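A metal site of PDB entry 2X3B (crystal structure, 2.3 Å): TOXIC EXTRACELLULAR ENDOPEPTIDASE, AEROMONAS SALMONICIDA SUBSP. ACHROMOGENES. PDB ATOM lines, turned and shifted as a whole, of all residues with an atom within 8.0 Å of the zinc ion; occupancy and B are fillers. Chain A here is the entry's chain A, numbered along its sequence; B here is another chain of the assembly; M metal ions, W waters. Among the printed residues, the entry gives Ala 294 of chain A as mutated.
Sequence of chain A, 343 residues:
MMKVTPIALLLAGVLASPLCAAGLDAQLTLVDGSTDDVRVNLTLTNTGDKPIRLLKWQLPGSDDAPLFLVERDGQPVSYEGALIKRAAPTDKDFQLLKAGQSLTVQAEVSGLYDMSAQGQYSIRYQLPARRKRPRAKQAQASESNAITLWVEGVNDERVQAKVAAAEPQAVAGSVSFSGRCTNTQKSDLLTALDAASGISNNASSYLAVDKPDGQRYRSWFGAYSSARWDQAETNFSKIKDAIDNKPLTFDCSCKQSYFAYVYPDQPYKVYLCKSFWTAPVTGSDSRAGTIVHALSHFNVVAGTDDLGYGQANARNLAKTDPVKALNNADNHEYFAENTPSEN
OH of Tyr 309 sits at hydrogen-bond distance from O of Ile 84 of chain B, at 2.8 Å.
A ring nitrogen (ND1) of His 293 is in hydrogen-bond range of the side-chain carboxylate of Asp 330.
The side-chain amino group (NZ) of Lys 85 of chain B is in salt-bridge range of the side-chain carboxylate (OD1) of Asp 330 (3.1 Å).
The backbone carbonyl oxygen (O) of Lys 85 of chain B sits at hydrogen-bond distance from the backbone NH (N) of Phe 259 (3.0 Å).
A ring nitrogen (ND1) of His 297 sits at hydrogen-bond distance from the backbone carbonyl oxygen of Thr 304 (2.9 Å).
OD2 of Asp 306 lies close to N of Ile 84 of chain B (3.2 Å).
OE1 of Glu 333 is in salt-bridge range of NZ of Lys 85 of chain B (2.9 Å).
The backbone NH (N) of Lys 85 of chain B lies within hydrogen-bond range of the backbone carbonyl oxygen (O) of Ala 260 (2.9 Å).
Ile 84 of chain B touches the zinc ion.
Lys 85 of chain B touches the zinc ion (N to ZN, 3.5 Å).
Within 4 Å of the zinc ion: His 293, His 297, Asp 306, Ile 84 of chain B and Lys 85 of chain B.
The zinc ion is bound by the side-chain carboxylate of Asp 306 (1.9 Å), a ring nitrogen (NE2) of His 297 (2.0 Å), a ring nitrogen (NE2) of His 293 (2.1 Å) and water W1 (2.4 Å).
Slightly farther from the zinc ion lies OD1 of Asp 306 (2.8 Å).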
ATOM      1  N   PHE A 259      19.569   5.432  13.124  1.00  0.00           N
ATOM      2  CA  PHE A 259      19.522   5.502  11.669  1.00  0.00           C
ATOM      3  C   PHE A 259      20.883   5.425  10.992  1.00  0.00           C
ATOM      4  O   PHE A 259      21.117   4.563  10.147  1.00  0.00           O
ATOM      5  CB  PHE A 259      18.815   6.780  11.223  1.00  0.00           C
ATOM      6  CG  PHE A 259      17.320   6.694  11.222  1.00  0.00           C
ATOM      7  CD1 PHE A 259      16.634   6.488  10.031  1.00  0.00           C
ATOM      8  CD2 PHE A 259      16.597   6.840  12.397  1.00  0.00           C
ATOM      9  CE1 PHE A 259      15.247   6.412  10.019  1.00  0.00           C
ATOM     10  CE2 PHE A 259      15.216   6.749  12.396  1.00  0.00           C
ATOM     11  CZ  PHE A 259      14.539   6.543  11.201  1.00  0.00           C
ATOM     12  N   ALA A 260      21.766   6.357  11.350  1.00  0.00           N
ATOM     13  CA  ALA A 260      23.044   6.530  10.674  1.00  0.00           C
ATOM     14  C   ALA A 260      23.933   7.437  11.515  1.00  0.00           C
ATOM     15  O   ALA A 260      23.464   8.066  12.464  1.00  0.00           O
ATOM     16  CB  ALA A 260      22.835   7.144   9.270  1.00  0.00           C
ATOM     17  N   TYR A 261      25.212   7.490  11.174  1.00  0.00           N
ATOM     18  CA  TYR A 261      26.131   8.436  11.781  1.00  0.00           C
ATOM     19  C   TYR A 261      27.267   8.821  10.821  1.00  0.00           C
ATOM     20  O   TYR A 261      27.541   8.109   9.855  1.00  0.00           O
ATOM     21  CB  TYR A 261      26.689   7.937  13.125  1.00  0.00           C
ATOM     22  CG  TYR A 261      27.647   6.780  13.054  1.00  0.00           C
ATOM     23  CD1 TYR A 261      29.017   6.988  12.887  1.00  0.00           C
ATOM     24  CD2 TYR A 261      27.193   5.472  13.192  1.00  0.00           C
ATOM     25  CE1 TYR A 261      29.912   5.918  12.840  1.00  0.00           C
ATOM     26  CE2 TYR A 261      28.075   4.396  13.143  1.00  0.00           C
ATOM     27  CZ  TYR A 261      29.427   4.626  12.964  1.00  0.00           C
ATOM     28  OH  TYR A 261      30.293   3.551  12.907  1.00  0.00           O
ATOM     29  N   VAL A 262      27.904   9.949  11.099  1.00  0.00           N
ATOM     30  CA  VAL A 262      29.020  10.416  10.284  1.00  0.00           C
ATOM     31  C   VAL A 262      30.046  11.082  11.175  1.00  0.00           C
ATOM     32  O   VAL A 262      29.713  11.575  12.252  1.00  0.00           O
ATOM     33  CB  VAL A 262      28.575  11.442   9.193  1.00  0.00           C
ATOM     34  CG1 VAL A 262      27.724  10.773   8.122  1.00  0.00           C
ATOM     35  CG2 VAL A 262      27.836  12.642   9.816  1.00  0.00           C
ATOM     36  N   THR A 290      17.458  10.164   5.202  1.00  0.00           N
ATOM     37  CA  THR A 290      18.628   9.890   6.051  1.00  0.00           C
ATOM     38  C   THR A 290      19.906  10.278   5.303  1.00  0.00           C
ATOM     39  O   THR A 290      20.805  10.872   5.873  1.00  0.00           O
ATOM     40  CB  THR A 290      18.658   8.399   6.509  1.00  0.00           C
ATOM     41  OG1 THR A 290      17.557   8.136   7.382  1.00  0.00           O
ATOM     42  CG2 THR A 290      19.940   8.075   7.236  1.00  0.00           C
ATOM     43  N   HIS A 293      20.131  13.997   5.387  1.00  0.00           N
ATOM     44  CA  HIS A 293      20.535  14.290   6.764  1.00  0.00           C
ATOM     45  C   HIS A 293      22.047  14.130   6.972  1.00  0.00           C
ATOM     46  O   HIS A 293      22.719  15.061   7.425  1.00  0.00           O
ATOM     47  CB  HIS A 293      19.779  13.366   7.714  1.00  0.00           C
ATOM     48  CG  HIS A 293      20.202  13.486   9.154  1.00  0.00           C
ATOM     49  ND1 HIS A 293      19.366  13.981  10.132  1.00  0.00           N
ATOM     50  CD2 HIS A 293      21.356  13.169   9.774  1.00  0.00           C
ATOM     51  CE1 HIS A 293      19.984  13.958  11.293  1.00  0.00           C
ATOM     52  NE2 HIS A 293      21.203  13.479  11.099  1.00  0.00           N
ATOM     53  N   ALA A 294      22.566  12.947   6.651  1.00  0.00           N
ATOM     54  CA  ALA A 294      23.953  12.620   6.971  1.00  0.00           C
ATOM     55  C   ALA A 294      24.933  13.453   6.159  1.00  0.00           C
ATOM     56  O   ALA A 294      25.933  13.924   6.690  1.00  0.00           O
ATOM     57  CB  ALA A 294      24.225  11.126   6.798  1.00  0.00           C
ATOM     58  N   LEU A 295      24.635  13.657   4.883  1.00  0.00           N
ATOM     59  CA  LEU A 295      25.519  14.453   4.026  1.00  0.00           C
ATOM     60  C   LEU A 295      25.600  15.913   4.421  1.00  0.00           C
ATOM     61  O   LEU A 295      26.654  16.530   4.304  1.00  0.00           O
ATOM     62  CB  LEU A 295      25.127  14.311   2.560  1.00  0.00           C
ATOM     63  CG  LEU A 295      25.447  12.975   1.873  1.00  0.00           C
ATOM     64  CD1 LEU A 295      24.808  12.933   0.493  1.00  0.00           C
ATOM     65  CD2 LEU A 295      26.967  12.729   1.772  1.00  0.00           C
ATOM     66  N   SER A 296      24.493  16.480   4.913  1.00  0.00           N
ATOM     67  CA  SER A 296      24.471  17.879   5.371  1.00  0.00           C
ATOM     68  C   SER A 296      25.484  18.152   6.486  1.00  0.00           C
ATOM     69  O   SER A 296      25.969  19.283   6.615  1.00  0.00           O
ATOM     70  CB  SER A 296      23.050  18.298   5.781  1.00  0.00           C
ATOM     71  OG  SER A 296      22.726  17.893   7.104  1.00  0.00           O
ATOM     72  N   HIS A 297      25.805  17.123   7.274  1.00  0.00           N
ATOM     73  CA  HIS A 297      26.763  17.242   8.381  1.00  0.00           C
ATOM     74  C   HIS A 297      28.172  17.617   7.948  1.00  0.00           C
ATOM     75  O   HIS A 297      28.836  18.410   8.618  1.00  0.00           O
ATOM     76  CB  HIS A 297      26.867  15.939   9.164  1.00  0.00           C
ATOM     77  CG  HIS A 297      25.675  15.637  10.021  1.00  0.00           C
ATOM     78  ND1 HIS A 297      25.245  16.490  11.007  1.00  0.00           N
ATOM     79  CD2 HIS A 297      24.863  14.559  10.061  1.00  0.00           C
ATOM     80  CE1 HIS A 297      24.193  15.961  11.613  1.00  0.00           C
ATOM     81  NE2 HIS A 297      23.949  14.788  11.055  1.00  0.00           N
ATOM     82  N   THR A 304      26.125  21.024   9.211  1.00  0.00           N
ATOM     83  CA  THR A 304      24.999  21.071  10.145  1.00  0.00           C
ATOM     84  C   THR A 304      25.285  20.239  11.391  1.00  0.00           C
ATOM     85  O   THR A 304      26.065  19.280  11.340  1.00  0.00           O
ATOM     86  CB  THR A 304      23.703  20.545   9.501  1.00  0.00           C
ATOM     87  OG1 THR A 304      23.898  19.187   9.102  1.00  0.00           O
ATOM     88  CG2 THR A 304      23.338  21.388   8.276  1.00  0.00           C
ATOM     89  N   ASP A 305      24.640  20.602  12.491  1.00  0.00           N
ATOM     90  CA  ASP A 305      24.742  19.835  13.713  1.00  0.00           C
ATOM     91  C   ASP A 305      23.512  18.941  13.900  1.00  0.00           C
ATOM     92  O   ASP A 305      22.604  18.955  13.079  1.00  0.00           O
ATOM     93  CB  ASP A 305      24.953  20.762  14.919  1.00  0.00           C
ATOM     94  CG  ASP A 305      26.411  21.171  15.102  1.00  0.00           C
ATOM     95  OD1 ASP A 305      27.296  20.293  15.028  1.00  0.00           O
ATOM     96  OD2 ASP A 305      26.677  22.372  15.349  1.00  0.00           O
ATOM     97  N   ASP A 306      23.518  18.145  14.972  1.00  0.00           N
ATOM     98  CA  ASP A 306      22.351  17.350  15.346  1.00  0.00           C
ATOM     99  C   ASP A 306      21.825  17.867  16.671  1.00  0.00           C
ATOM    100  O   ASP A 306      21.923  17.196  17.697  1.00  0.00           O
ATOM    101  CB  ASP A 306      22.692  15.869  15.420  1.00  0.00           C
ATOM    102  CG  ASP A 306      22.437  15.137  14.126  1.00  0.00           C
ATOM    103  OD1 ASP A 306      21.642  15.642  13.297  1.00  0.00           O
ATOM    104  OD2 ASP A 306      23.014  14.048  13.923  1.00  0.00           O
ATOM    105  N   LEU A 307      21.277  19.080  16.612  1.00  0.00           N
ATOM    106  CA  LEU A 307      20.753  19.799  17.766  1.00  0.00           C
ATOM    107  C   LEU A 307      19.481  19.168  18.312  1.00  0.00           C
ATOM    108  O   LEU A 307      19.217  19.258  19.511  1.00  0.00           O
ATOM    109  CB  LEU A 307      20.483  21.270  17.392  1.00  0.00           C
ATOM    110  CG  LEU A 307      21.620  22.071  16.759  1.00  0.00           C
ATOM    111  CD1 LEU A 307      21.094  23.360  16.163  1.00  0.00           C
ATOM    112  CD2 LEU A 307      22.736  22.370  17.769  1.00  0.00           C
ATOM    113  N   GLY A 308      18.686  18.562  17.440  1.00  0.00           N
ATOM    114  CA  GLY A 308      17.440  17.911  17.850  1.00  0.00           C
ATOM    115  C   GLY A 308      16.924  16.929  16.820  1.00  0.00           C
ATOM    116  O   GLY A 308      17.285  17.018  15.640  1.00  0.00           O
ATOM    117  N   TYR A 309      16.089  15.992  17.262  1.00  0.00           N
ATOM    118  CA  TYR A 309      15.623  14.912  16.387  1.00  0.00           C
ATOM    119  C   TYR A 309      14.101  14.773  16.300  1.00  0.00           C
ATOM    120  O   TYR A 309      13.394  14.879  17.302  1.00  0.00           O
ATOM    121  CB  TYR A 309      16.200  13.576  16.830  1.00  0.00           C
ATOM    122  CG  TYR A 309      17.699  13.559  16.986  1.00  0.00           C
ATOM    123  CD1 TYR A 309      18.543  13.506  15.878  1.00  0.00           C
ATOM    124  CD2 TYR A 309      18.266  13.578  18.260  1.00  0.00           C
ATOM    125  CE1 TYR A 309      19.915  13.487  16.033  1.00  0.00           C
ATOM    126  CE2 TYR A 309      19.641  13.552  18.420  1.00  0.00           C
ATOM    127  CZ  TYR A 309      20.464  13.506  17.316  1.00  0.00           C
ATOM    128  OH  TYR A 309      21.828  13.481  17.499  1.00  0.00           O
ATOM    129  N   ASN A 328      20.612  22.427  11.579  1.00  0.00           N
ATOM    130  CA  ASN A 328      20.201  21.117  12.059  1.00  0.00           C
ATOM    131  C   ASN A 328      19.884  20.214  10.889  1.00  0.00           C
ATOM    132  O   ASN A 328      19.074  20.572  10.021  1.00  0.00           O
ATOM    133  CB  ASN A 328      18.998  21.203  12.997  1.00  0.00           C
ATOM    134  CG  ASN A 328      18.771  19.913  13.804  1.00  0.00           C
ATOM    135  OD1 ASN A 328      19.696  19.414  14.455  1.00  0.00           O
ATOM    136  ND2 ASN A 328      17.547  19.406  13.777  1.00  0.00           N
ATOM    137  N   ALA A 329      20.523  19.041  10.883  1.00  0.00           N
ATOM    138  CA  ALA A 329      20.394  18.065   9.807  1.00  0.00           C
ATOM    139  C   ALA A 329      18.964  17.607   9.533  1.00  0.00           C
ATOM    140  O   ALA A 329      18.532  17.566   8.378  1.00  0.00           O
ATOM    141  CB  ALA A 329      21.299  16.860  10.072  1.00  0.00           C
ATOM    142  N   ASP A 330      18.234  17.253  10.600  1.00  0.00           N
ATOM    143  CA  ASP A 330      16.846  16.804  10.481  1.00  0.00           C
ATOM    144  C   ASP A 330      15.957  17.875   9.844  1.00  0.00           C
ATOM    145  O   ASP A 330      15.066  17.554   9.071  1.00  0.00           O
ATOM    146  CB  ASP A 330      16.287  16.366  11.837  1.00  0.00           C
ATOM    147  CG  ASP A 330      16.356  14.872  12.039  1.00  0.00           C
ATOM    148  OD1 ASP A 330      16.825  14.143  11.134  1.00  0.00           O
ATOM    149  OD2 ASP A 330      15.924  14.392  13.111  1.00  0.00           O
ATOM    150  N   GLU A 333      16.535  17.491   6.257  1.00  0.00           N
ATOM    151  CA  GLU A 333      15.898  16.239   5.843  1.00  0.00           C
ATOM    152  C   GLU A 333      14.392  16.420   5.625  1.00  0.00           C
ATOM    153  O   GLU A 333      13.877  16.104   4.561  1.00  0.00           O
ATOM    154  CB  GLU A 333      16.155  15.136   6.890  1.00  0.00           C
ATOM    155  CG  GLU A 333      15.318  13.888   6.670  1.00  0.00           C
ATOM    156  CD  GLU A 333      15.707  12.719   7.566  1.00  0.00           C
ATOM    157  OE1 GLU A 333      16.616  12.853   8.401  1.00  0.00           O
ATOM    158  OE2 GLU A 333      15.096  11.650   7.414  1.00  0.00           O
ATOM    159  N   ALA B  82      31.443  11.636  16.429  1.00  0.00           N
ATOM    160  CA  ALA B  82      30.409  11.354  15.462  1.00  0.00           C
ATOM    161  C   ALA B  82      29.146  12.158  15.745  1.00  0.00           C
ATOM    162  O   ALA B  82      28.903  12.575  16.882  1.00  0.00           O
ATOM    163  CB  ALA B  82      30.093   9.867  15.426  1.00  0.00           C
ATOM    164  N   LEU B  83      28.378  12.383  14.693  1.00  0.00           N
ATOM    165  CA  LEU B  83      27.053  12.990  14.733  1.00  0.00           C
ATOM    166  C   LEU B  83      26.113  11.871  14.325  1.00  0.00           C
ATOM    167  O   LEU B  83      26.415  11.114  13.391  1.00  0.00           O
ATOM    168  CB  LEU B  83      26.991  14.141  13.726  1.00  0.00           C
ATOM    169  CG  LEU B  83      27.086  15.630  14.081  1.00  0.00           C
ATOM    170  CD1 LEU B  83      27.584  15.981  15.481  1.00  0.00           C
ATOM    171  CD2 LEU B  83      27.931  16.325  13.038  1.00  0.00           C
ATOM    172  N   ILE B  84      24.971  11.762  14.993  1.00  0.00           N
ATOM    173  CA  ILE B  84      24.137  10.575  14.879  1.00  0.00           C
ATOM    174  C   ILE B  84      22.683  10.946  14.599  1.00  0.00           C
ATOM    175  O   ILE B  84      22.111  11.762  15.315  1.00  0.00           O
ATOM    176  CB  ILE B  84      24.212   9.736  16.178  1.00  0.00           C
ATOM    177  CG1 ILE B  84      25.638   9.239  16.434  1.00  0.00           C
ATOM    178  CG2 ILE B  84      23.256   8.552  16.132  1.00  0.00           C
ATOM    179  CD1 ILE B  84      25.886   8.715  17.862  1.00  0.00           C
ATOM    180  N   LYS B  85      22.100  10.357  13.553  1.00  0.00           N
ATOM    181  CA  LYS B  85      20.665  10.479  13.341  1.00  0.00           C
ATOM    182  C   LYS B  85      19.918   9.464  14.208  1.00  0.00           C
ATOM    183  O   LYS B  85      19.959   8.265  13.936  1.00  0.00           O
ATOM    184  CB  LYS B  85      20.269  10.330  11.868  1.00  0.00           C
ATOM    185  CG  LYS B  85      18.757  10.440  11.683  1.00  0.00           C
ATOM    186  CD  LYS B  85      18.325  10.433  10.221  1.00  0.00           C
ATOM    187  CE  LYS B  85      16.841  10.137  10.107  1.00  0.00           C
ATOM    188  NZ  LYS B  85      15.970  11.216  10.685  1.00  0.00           N
ATOM    189  N   ARG B  86      19.265   9.964  15.246  1.00  0.00           N
ATOM    190  CA  ARG B  86      18.434   9.151  16.137  1.00  0.00           C
ATOM    191  C   ARG B  86      16.968   9.480  15.879  1.00  0.00           C
ATOM    192  O   ARG B  86      16.644  10.586  15.470  1.00  0.00           O
ATOM    193  CB  ARG B  86      18.728   9.481  17.602  1.00  0.00           C
ATOM    194  CG  ARG B  86      20.183   9.560  17.982  1.00  0.00           C
ATOM    195  CD  ARG B  86      20.294  10.084  19.397  1.00  0.00           C
ATOM    196  NE  ARG B  86      21.610   9.817  19.977  1.00  0.00           N
ATOM    197  CZ  ARG B  86      21.902   8.734  20.697  1.00  0.00           C
ATOM    198  NH1 ARG B  86      20.975   7.819  20.931  1.00  0.00           N
ATOM    199  NH2 ARG B  86      23.128   8.573  21.170  1.00  0.00           N
HETATM  200 ZN    ZN M   1      23.003  13.452  12.117  1.00  0.00          ZN
HETATM  201  O   HOH W   1      24.036  11.489  11.221  1.00  0.00           O
